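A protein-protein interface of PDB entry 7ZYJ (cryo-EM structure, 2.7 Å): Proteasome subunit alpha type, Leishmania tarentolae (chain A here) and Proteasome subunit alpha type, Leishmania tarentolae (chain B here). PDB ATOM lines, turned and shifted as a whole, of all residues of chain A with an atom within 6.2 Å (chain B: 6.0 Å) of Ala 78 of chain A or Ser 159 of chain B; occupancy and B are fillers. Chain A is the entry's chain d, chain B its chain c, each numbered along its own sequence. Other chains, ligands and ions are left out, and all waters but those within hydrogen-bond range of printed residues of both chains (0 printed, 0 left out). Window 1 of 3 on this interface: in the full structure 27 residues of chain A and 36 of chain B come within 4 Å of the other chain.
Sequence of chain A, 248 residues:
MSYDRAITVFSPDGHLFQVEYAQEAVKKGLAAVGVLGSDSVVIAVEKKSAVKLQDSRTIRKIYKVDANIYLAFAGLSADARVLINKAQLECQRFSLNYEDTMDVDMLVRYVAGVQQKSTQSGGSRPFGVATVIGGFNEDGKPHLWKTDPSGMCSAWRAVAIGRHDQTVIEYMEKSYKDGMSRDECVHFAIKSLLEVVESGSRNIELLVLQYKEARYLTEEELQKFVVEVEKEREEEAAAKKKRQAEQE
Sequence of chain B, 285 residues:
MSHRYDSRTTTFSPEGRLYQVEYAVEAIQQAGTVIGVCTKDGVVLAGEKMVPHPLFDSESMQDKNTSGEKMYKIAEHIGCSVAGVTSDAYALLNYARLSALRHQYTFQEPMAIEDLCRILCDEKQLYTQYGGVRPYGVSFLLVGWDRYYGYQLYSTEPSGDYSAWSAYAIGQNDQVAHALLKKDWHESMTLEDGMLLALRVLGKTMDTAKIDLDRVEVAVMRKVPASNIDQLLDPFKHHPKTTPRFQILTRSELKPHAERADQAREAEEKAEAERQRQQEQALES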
ATOM      1  N   PHE A  73      32.938  -4.596 -10.665  1.00  0.00           N
ATOM      2  CA  PHE A  73      32.320  -5.739 -10.009  1.00  0.00           C
ATOM      3  C   PHE A  73      32.164  -6.905 -10.975  1.00  0.00           C
ATOM      4  O   PHE A  73      32.185  -6.749 -12.198  1.00  0.00           O
ATOM      5  CB  PHE A  73      30.951  -5.379  -9.412  1.00  0.00           C
ATOM      6  CG  PHE A  73      29.867  -5.196 -10.438  1.00  0.00           C
ATOM      7  CD1 PHE A  73      29.629  -3.956 -11.003  1.00  0.00           C
ATOM      8  CD2 PHE A  73      29.072  -6.265 -10.825  1.00  0.00           C
ATOM      9  CE1 PHE A  73      28.630  -3.790 -11.940  1.00  0.00           C
ATOM     10  CE2 PHE A  73      28.073  -6.103 -11.760  1.00  0.00           C
ATOM     11  CZ  PHE A  73      27.851  -4.864 -12.318  1.00  0.00           C
ATOM     12  N   LEU A  76      26.131 -10.326  -9.615  1.00  0.00           N
ATOM     13  CA  LEU A  76      24.793  -9.800  -9.847  1.00  0.00           C
ATOM     14  C   LEU A  76      24.831  -8.278  -9.906  1.00  0.00           C
ATOM     15  O   LEU A  76      25.398  -7.627  -9.024  1.00  0.00           O
ATOM     16  CB  LEU A  76      23.840 -10.269  -8.748  1.00  0.00           C
ATOM     17  CG  LEU A  76      23.810 -11.777  -8.489  1.00  0.00           C
ATOM     18  CD1 LEU A  76      22.750 -12.128  -7.459  1.00  0.00           C
ATOM     19  CD2 LEU A  76      23.573 -12.539  -9.783  1.00  0.00           C
ATOM     20  N   SER A  77      24.224  -7.715 -10.953  1.00  0.00           N
ATOM     21  CA  SER A  77      24.327  -6.279 -11.191  1.00  0.00           C
ATOM     22  C   SER A  77      23.561  -5.472 -10.149  1.00  0.00           C
ATOM     23  O   SER A  77      24.020  -4.406  -9.724  1.00  0.00           O
ATOM     24  CB  SER A  77      23.830  -5.946 -12.597  1.00  0.00           C
ATOM     25  OG  SER A  77      24.633  -6.573 -13.580  1.00  0.00           O
ATOM     26  N   ALA A  78      22.388  -5.953  -9.732  1.00  0.00           N
ATOM     27  CA  ALA A  78      21.568  -5.181  -8.801  1.00  0.00           C
ATOM     28  C   ALA A  78      22.173  -5.165  -7.402  1.00  0.00           C
ATOM     29  O   ALA A  78      22.192  -4.121  -6.735  1.00  0.00           O
ATOM     30  CB  ALA A  78      20.148  -5.743  -8.773  1.00  0.00           C
ATOM     31  N   ASP A  79      22.673  -6.313  -6.940  1.00  0.00           N
ATOM     32  CA  ASP A  79      23.382  -6.345  -5.666  1.00  0.00           C
ATOM     33  C   ASP A  79      24.622  -5.464  -5.717  1.00  0.00           C
ATOM     34  O   ASP A  79      24.958  -4.787  -4.738  1.00  0.00           O
ATOM     35  CB  ASP A  79      23.759  -7.781  -5.307  1.00  0.00           C
ATOM     36  CG  ASP A  79      22.552  -8.642  -5.001  1.00  0.00           C
ATOM     37  OD1 ASP A  79      21.493  -8.083  -4.645  1.00  0.00           O
ATOM     38  OD2 ASP A  79      22.661  -9.880  -5.111  1.00  0.00           O
ATOM     39  N   ALA A  80      25.314  -5.459  -6.859  1.00  0.00           N
ATOM     40  CA  ALA A  80      26.473  -4.593  -7.022  1.00  0.00           C
ATOM     41  C   ALA A  80      26.083  -3.124  -6.943  1.00  0.00           C
ATOM     42  O   ALA A  80      26.804  -2.317  -6.350  1.00  0.00           O
ATOM     43  CB  ALA A  80      27.165  -4.889  -8.347  1.00  0.00           C
ATOM     44  N   ARG A  81      24.954  -2.754  -7.550  1.00  0.00           N
ATOM     45  CA  ARG A  81      24.495  -1.372  -7.471  1.00  0.00           C
ATOM     46  C   ARG A  81      24.152  -0.986  -6.039  1.00  0.00           C
ATOM     47  O   ARG A  81      24.464   0.128  -5.598  1.00  0.00           O
ATOM     48  CB  ARG A  81      23.291  -1.160  -8.387  1.00  0.00           C
ATOM     49  CG  ARG A  81      22.927   0.301  -8.591  1.00  0.00           C
ATOM     50  CD  ARG A  81      21.489   0.451  -9.047  1.00  0.00           C
ATOM     51  NE  ARG A  81      21.113  -0.602  -9.981  1.00  0.00           N
ATOM     52  CZ  ARG A  81      20.087  -1.424  -9.812  1.00  0.00           C
ATOM     53  NH1 ARG A  81      19.301  -1.341  -8.753  1.00  0.00           N
ATOM     54  NH2 ARG A  81      19.848  -2.356 -10.730  1.00  0.00           N
ATOM     55  N   VAL A  82      23.509  -1.891  -5.299  1.00  0.00           N
ATOM     56  CA  VAL A  82      23.214  -1.621  -3.893  1.00  0.00           C
ATOM     57  C   VAL A  82      24.504  -1.423  -3.104  1.00  0.00           C
ATOM     58  O   VAL A  82      24.624  -0.491  -2.296  1.00  0.00           O
ATOM     59  CB  VAL A  82      22.354  -2.754  -3.304  1.00  0.00           C
ATOM     60  CG1 VAL A  82      22.253  -2.622  -1.793  1.00  0.00           C
ATOM     61  CG2 VAL A  82      20.972  -2.743  -3.932  1.00  0.00           C
ATOM     62  N   LEU A  83      25.492  -2.290  -3.336  1.00  0.00           N
ATOM     63  CA  LEU A  83      26.771  -2.175  -2.641  1.00  0.00           C
ATOM     64  C   LEU A  83      27.482  -0.872  -2.992  1.00  0.00           C
ATOM     65  O   LEU A  83      28.080  -0.230  -2.121  1.00  0.00           O
ATOM     66  CB  LEU A  83      27.651  -3.377  -2.978  1.00  0.00           C
ATOM     67  CG  LEU A  83      28.547  -3.913  -1.864  1.00  0.00           C
ATOM     68  CD1 LEU A  83      27.710  -4.341  -0.672  1.00  0.00           C
ATOM     69  CD2 LEU A  83      29.383  -5.072  -2.376  1.00  0.00           C
ATOM     70  N   PHE A 127      25.491 -11.121  -0.529  1.00  0.00           N
ATOM     71  CA  PHE A 127      25.679 -10.470  -1.819  1.00  0.00           C
ATOM     72  C   PHE A 127      26.448 -11.389  -2.758  1.00  0.00           C
ATOM     73  O   PHE A 127      27.468 -11.972  -2.376  1.00  0.00           O
ATOM     74  CB  PHE A 127      26.431  -9.151  -1.650  1.00  0.00           C
ATOM     75  CG  PHE A 127      25.598  -8.038  -1.086  1.00  0.00           C
ATOM     76  CD1 PHE A 127      24.800  -7.267  -1.911  1.00  0.00           C
ATOM     77  CD2 PHE A 127      25.629  -7.749   0.265  1.00  0.00           C
ATOM     78  CE1 PHE A 127      24.037  -6.238  -1.395  1.00  0.00           C
ATOM     79  CE2 PHE A 127      24.868  -6.723   0.787  1.00  0.00           C
ATOM     80  CZ  PHE A 127      24.072  -5.966  -0.043  1.00  0.00           C
ATOM     81  N   VAL A 129      28.404 -10.628  -5.214  1.00  0.00           N
ATOM     82  CA  VAL A 129      29.239  -9.654  -5.905  1.00  0.00           C
ATOM     83  C   VAL A 129      30.667  -9.764  -5.394  1.00  0.00           C
ATOM     84  O   VAL A 129      30.899  -9.868  -4.185  1.00  0.00           O
ATOM     85  CB  VAL A 129      28.710  -8.216  -5.710  1.00  0.00           C
ATOM     86  CG1 VAL A 129      29.586  -7.216  -6.445  1.00  0.00           C
ATOM     87  CG2 VAL A 129      27.271  -8.107  -6.178  1.00  0.00           C
ATOM     88  N   VAL B  21      13.478 -15.552  -9.002  1.00  0.00           N
ATOM     89  CA  VAL B  21      13.692 -14.556 -10.049  1.00  0.00           C
ATOM     90  C   VAL B  21      13.511 -15.181 -11.426  1.00  0.00           C
ATOM     91  O   VAL B  21      12.865 -14.601 -12.308  1.00  0.00           O
ATOM     92  CB  VAL B  21      15.083 -13.915  -9.897  1.00  0.00           C
ATOM     93  CG1 VAL B  21      15.392 -13.031 -11.091  1.00  0.00           C
ATOM     94  CG2 VAL B  21      15.159 -13.119  -8.605  1.00  0.00           C
ATOM     95  N   CYS B 121      14.056   0.071  -9.308  1.00  0.00           N
ATOM     96  CA  CYS B 121      14.785  -1.186  -9.420  1.00  0.00           C
ATOM     97  C   CYS B 121      15.333  -1.642  -8.077  1.00  0.00           C
ATOM     98  O   CYS B 121      15.422  -2.850  -7.827  1.00  0.00           O
ATOM     99  CB  CYS B 121      15.915  -1.053 -10.439  1.00  0.00           C
ATOM    100  SG  CYS B 121      15.366  -1.192 -12.148  1.00  0.00           S
ATOM    101  N   ASP B 122      15.710  -0.703  -7.206  1.00  0.00           N
ATOM    102  CA  ASP B 122      16.106  -1.080  -5.855  1.00  0.00           C
ATOM    103  C   ASP B 122      14.940  -1.686  -5.088  1.00  0.00           C
ATOM    104  O   ASP B 122      15.143  -2.583  -4.265  1.00  0.00           O
ATOM    105  CB  ASP B 122      16.665   0.128  -5.104  1.00  0.00           C
ATOM    106  CG  ASP B 122      17.637   0.937  -5.939  1.00  0.00           C
ATOM    107  OD1 ASP B 122      18.566   0.337  -6.520  1.00  0.00           O
ATOM    108  OD2 ASP B 122      17.472   2.171  -6.014  1.00  0.00           O
ATOM    109  N   LYS B 124      12.584  -3.583  -6.399  1.00  0.00           N
ATOM    110  CA  LYS B 124      12.491  -4.966  -6.850  1.00  0.00           C
ATOM    111  C   LYS B 124      13.645  -5.803  -6.311  1.00  0.00           C
ATOM    112  O   LYS B 124      13.454  -6.967  -5.941  1.00  0.00           O
ATOM    113  CB  LYS B 124      12.454  -5.015  -8.377  1.00  0.00           C
ATOM    114  CG  LYS B 124      11.381  -4.132  -8.986  1.00  0.00           C
ATOM    115  CD  LYS B 124      11.620  -3.894 -10.467  1.00  0.00           C
ATOM    116  CE  LYS B 124      11.079  -5.034 -11.308  1.00  0.00           C
ATOM    117  NZ  LYS B 124      10.999  -4.662 -12.745  1.00  0.00           N
ATOM    118  N   GLN B 125      14.850  -5.230  -6.263  1.00  0.00           N
ATOM    119  CA  GLN B 125      15.999  -5.962  -5.739  1.00  0.00           C
ATOM    120  C   GLN B 125      15.846  -6.277  -4.257  1.00  0.00           C
ATOM    121  O   GLN B 125      16.277  -7.343  -3.805  1.00  0.00           O
ATOM    122  CB  GLN B 125      17.283  -5.168  -5.972  1.00  0.00           C
ATOM    123  CG  GLN B 125      18.550  -5.946  -5.663  1.00  0.00           C
ATOM    124  CD  GLN B 125      19.021  -5.752  -4.237  1.00  0.00           C
ATOM    125  OE1 GLN B 125      18.554  -4.858  -3.533  1.00  0.00           O
ATOM    126  NE2 GLN B 125      19.949  -6.593  -3.802  1.00  0.00           N
ATOM    127  N   THR B 128      14.322  -9.545  -3.384  1.00  0.00           N
ATOM    128  CA  THR B 128      15.077 -10.735  -3.749  1.00  0.00           C
ATOM    129  C   THR B 128      16.196 -11.050  -2.766  1.00  0.00           C
ATOM    130  O   THR B 128      16.865 -12.075  -2.921  1.00  0.00           O
ATOM    131  CB  THR B 128      15.663 -10.584  -5.157  1.00  0.00           C
ATOM    132  OG1 THR B 128      16.766  -9.669  -5.123  1.00  0.00           O
ATOM    133  CG2 THR B 128      14.612 -10.062  -6.118  1.00  0.00           C
ATOM    134  N   TYR B 136       8.527  -9.293  -7.248  1.00  0.00           N
ATOM    135  CA  TYR B 136       7.552  -8.801  -8.212  1.00  0.00           C
ATOM    136  C   TYR B 136       7.784  -9.486  -9.553  1.00  0.00           C
ATOM    137  O   TYR B 136       8.906  -9.485 -10.069  1.00  0.00           O
ATOM    138  CB  TYR B 136       7.662  -7.286  -8.363  1.00  0.00           C
ATOM    139  CG  TYR B 136       7.375  -6.507  -7.102  1.00  0.00           C
ATOM    140  CD1 TYR B 136       6.078  -6.160  -6.756  1.00  0.00           C
ATOM    141  CD2 TYR B 136       8.406  -6.107  -6.264  1.00  0.00           C
ATOM    142  CE1 TYR B 136       5.813  -5.443  -5.607  1.00  0.00           C
ATOM    143  CE2 TYR B 136       8.152  -5.390  -5.114  1.00  0.00           C
ATOM    144  CZ  TYR B 136       6.854  -5.061  -4.790  1.00  0.00           C
ATOM    145  OH  TYR B 136       6.596  -4.347  -3.643  1.00  0.00           O
ATOM    146  N   GLU B 157      14.263  -5.765 -15.291  1.00  0.00           N
ATOM    147  CA  GLU B 157      14.033  -7.172 -15.021  1.00  0.00           C
ATOM    148  C   GLU B 157      13.493  -7.356 -13.611  1.00  0.00           C
ATOM    149  O   GLU B 157      13.677  -6.494 -12.747  1.00  0.00           O
ATOM    150  CB  GLU B 157      15.335  -7.963 -15.186  1.00  0.00           C
ATOM    151  CG  GLU B 157      16.064  -7.691 -16.490  1.00  0.00           C
ATOM    152  CD  GLU B 157      16.794  -8.912 -17.013  1.00  0.00           C
ATOM    153  OE1 GLU B 157      16.336 -10.042 -16.740  1.00  0.00           O
ATOM    154  OE2 GLU B 157      17.826  -8.744 -17.696  1.00  0.00           O
ATOM    155  N   PRO B 158      12.815  -8.476 -13.334  1.00  0.00           N
ATOM    156  CA  PRO B 158      12.318  -8.705 -11.971  1.00  0.00           C
ATOM    157  C   PRO B 158      13.410  -9.166 -11.020  1.00  0.00           C
ATOM    158  O   PRO B 158      13.213 -10.096 -10.232  1.00  0.00           O
ATOM    159  CB  PRO B 158      11.258  -9.795 -12.170  1.00  0.00           C
ATOM    160  CG  PRO B 158      11.730 -10.537 -13.362  1.00  0.00           C
ATOM    161  CD  PRO B 158      12.335  -9.505 -14.271  1.00  0.00           C
ATOM    162  N   SER B 159      14.569  -8.515 -11.089  1.00  0.00           N
ATOM    163  CA  SER B 159      15.667  -8.789 -10.176  1.00  0.00           C
ATOM    164  C   SER B 159      16.360  -7.526  -9.692  1.00  0.00           C
ATOM    165  O   SER B 159      17.288  -7.626  -8.883  1.00  0.00           O
ATOM    166  CB  SER B 159      16.702  -9.710 -10.840  1.00  0.00           C
ATOM    167  OG  SER B 159      17.294  -9.083 -11.963  1.00  0.00           O
ATOM    168  N   GLY B 160      15.942  -6.350 -10.152  1.00  0.00           N
ATOM    169  CA  GLY B 160      16.628  -5.113  -9.867  1.00  0.00           C
ATOM    170  C   GLY B 160      17.517  -4.619 -10.988  1.00  0.00           C
ATOM    171  O   GLY B 160      17.920  -3.451 -10.965  1.00  0.00           O
ATOM    172  N   ASP B 161      17.829  -5.466 -11.963  1.00  0.00           N
ATOM    173  CA  ASP B 161      18.666  -5.061 -13.083  1.00  0.00           C
ATOM    174  C   ASP B 161      17.867  -4.219 -14.068  1.00  0.00           C
ATOM    175  O   ASP B 161      16.689  -4.481 -14.319  1.00  0.00           O
ATOM    176  CB  ASP B 161      19.239  -6.286 -13.794  1.00  0.00           C
ATOM    177  CG  ASP B 161      20.160  -7.096 -12.907  1.00  0.00           C
ATOM    178  OD1 ASP B 161      20.681  -6.536 -11.920  1.00  0.00           O
ATOM    179  OD2 ASP B 161      20.365  -8.293 -13.198  1.00  0.00           O
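Printed residues of chain B within 4 Å of Arg 81 of chain A: Cys 121, Asp 122, Gly 160 and Asp 161. Lys 124 of chain B touches none of the printed residues of chain A. Thr 128 of chain B touches none of the printed residues of chain A. Of chain A, only Ala 78 comes within 4 Å of Ser 159 of chain B. Of the printed residues of chain A, Gly 160 of chain B touches Ala 78 and Arg 81. Printed residues of chain A within 4 Å of Asp 161 of chain B: Ser 77, Ala 78 and Arg 81. The nearest residue of chain B that does not touch Ala 78 of chain A is Cys 121 of chain B (5.6 Å). The nearest residue of chain A that does not touch Ser 159 of chain B is Asp 79 of chain A (5.9 Å).
Among the printed residues, pairs that only touch across the chains: Ser 77 of chain A with Asp 161 of chain B, Ala 78 of chain A with Gln 125 of chain B, Ala 78 of chain A with Ser 159 of chain B, Ala 78 of chain A with Gly 160 of chain B, Arg 81 of chain A with Cys 121 of chain B, Arg 81 of chain A with Asp 161 of chain B and Val 82 of chain A with Gln 125 of chain B.
Printed residues of chain A that touch a printed residue of chain B: Ser 77, Ala 78, Asp 79, Arg 81 and Val 82. Hydrophobic or aromatic side chains of chain A that line the printed part of chain B: Ala 78 and Val 82. Among the printed residues, 11 pairs touch across the chains. Among the printed residues, Asp or Glu carboxylates within 4 Å of a Lys or Arg side-chain nitrogen of the other chain: Arg 81 of chain A with Asp 122 of chain B.
O of Gly 160 of chain B sits close to NH1 of Arg 81 of chain A, at 3.4 Å. The backbone NH of Ala 78 of chain A sits at hydrogen-bond distance from the side-chain carboxylate of Asp 161 of chain B. OD1 of Asp 79 of chain A lies close to NE2 of Gln 125 of chain B (2.3 Å). The guanidinium group (NH1) of Arg 81 of chain A is in salt-bridge range of the side-chain carboxylate (OD1) of Asp 122 of chain B (2.9 Å).
The side-chain hydroxyl of Ser 159 of chain B lies within hydrogen-bond range of the side-chain carboxylate of Asp 161 of chain B (3.4 Å). The side-chain sulfur (SG) of Cys 121 of chain B lies close to the backbone carbonyl oxygen (O) of Gly 160 of chain B (3.6 Å). O of Gln 125 of chain B lies within hydrogen-bond range of OG1 of Thr 128 of chain B (2.7 Å).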
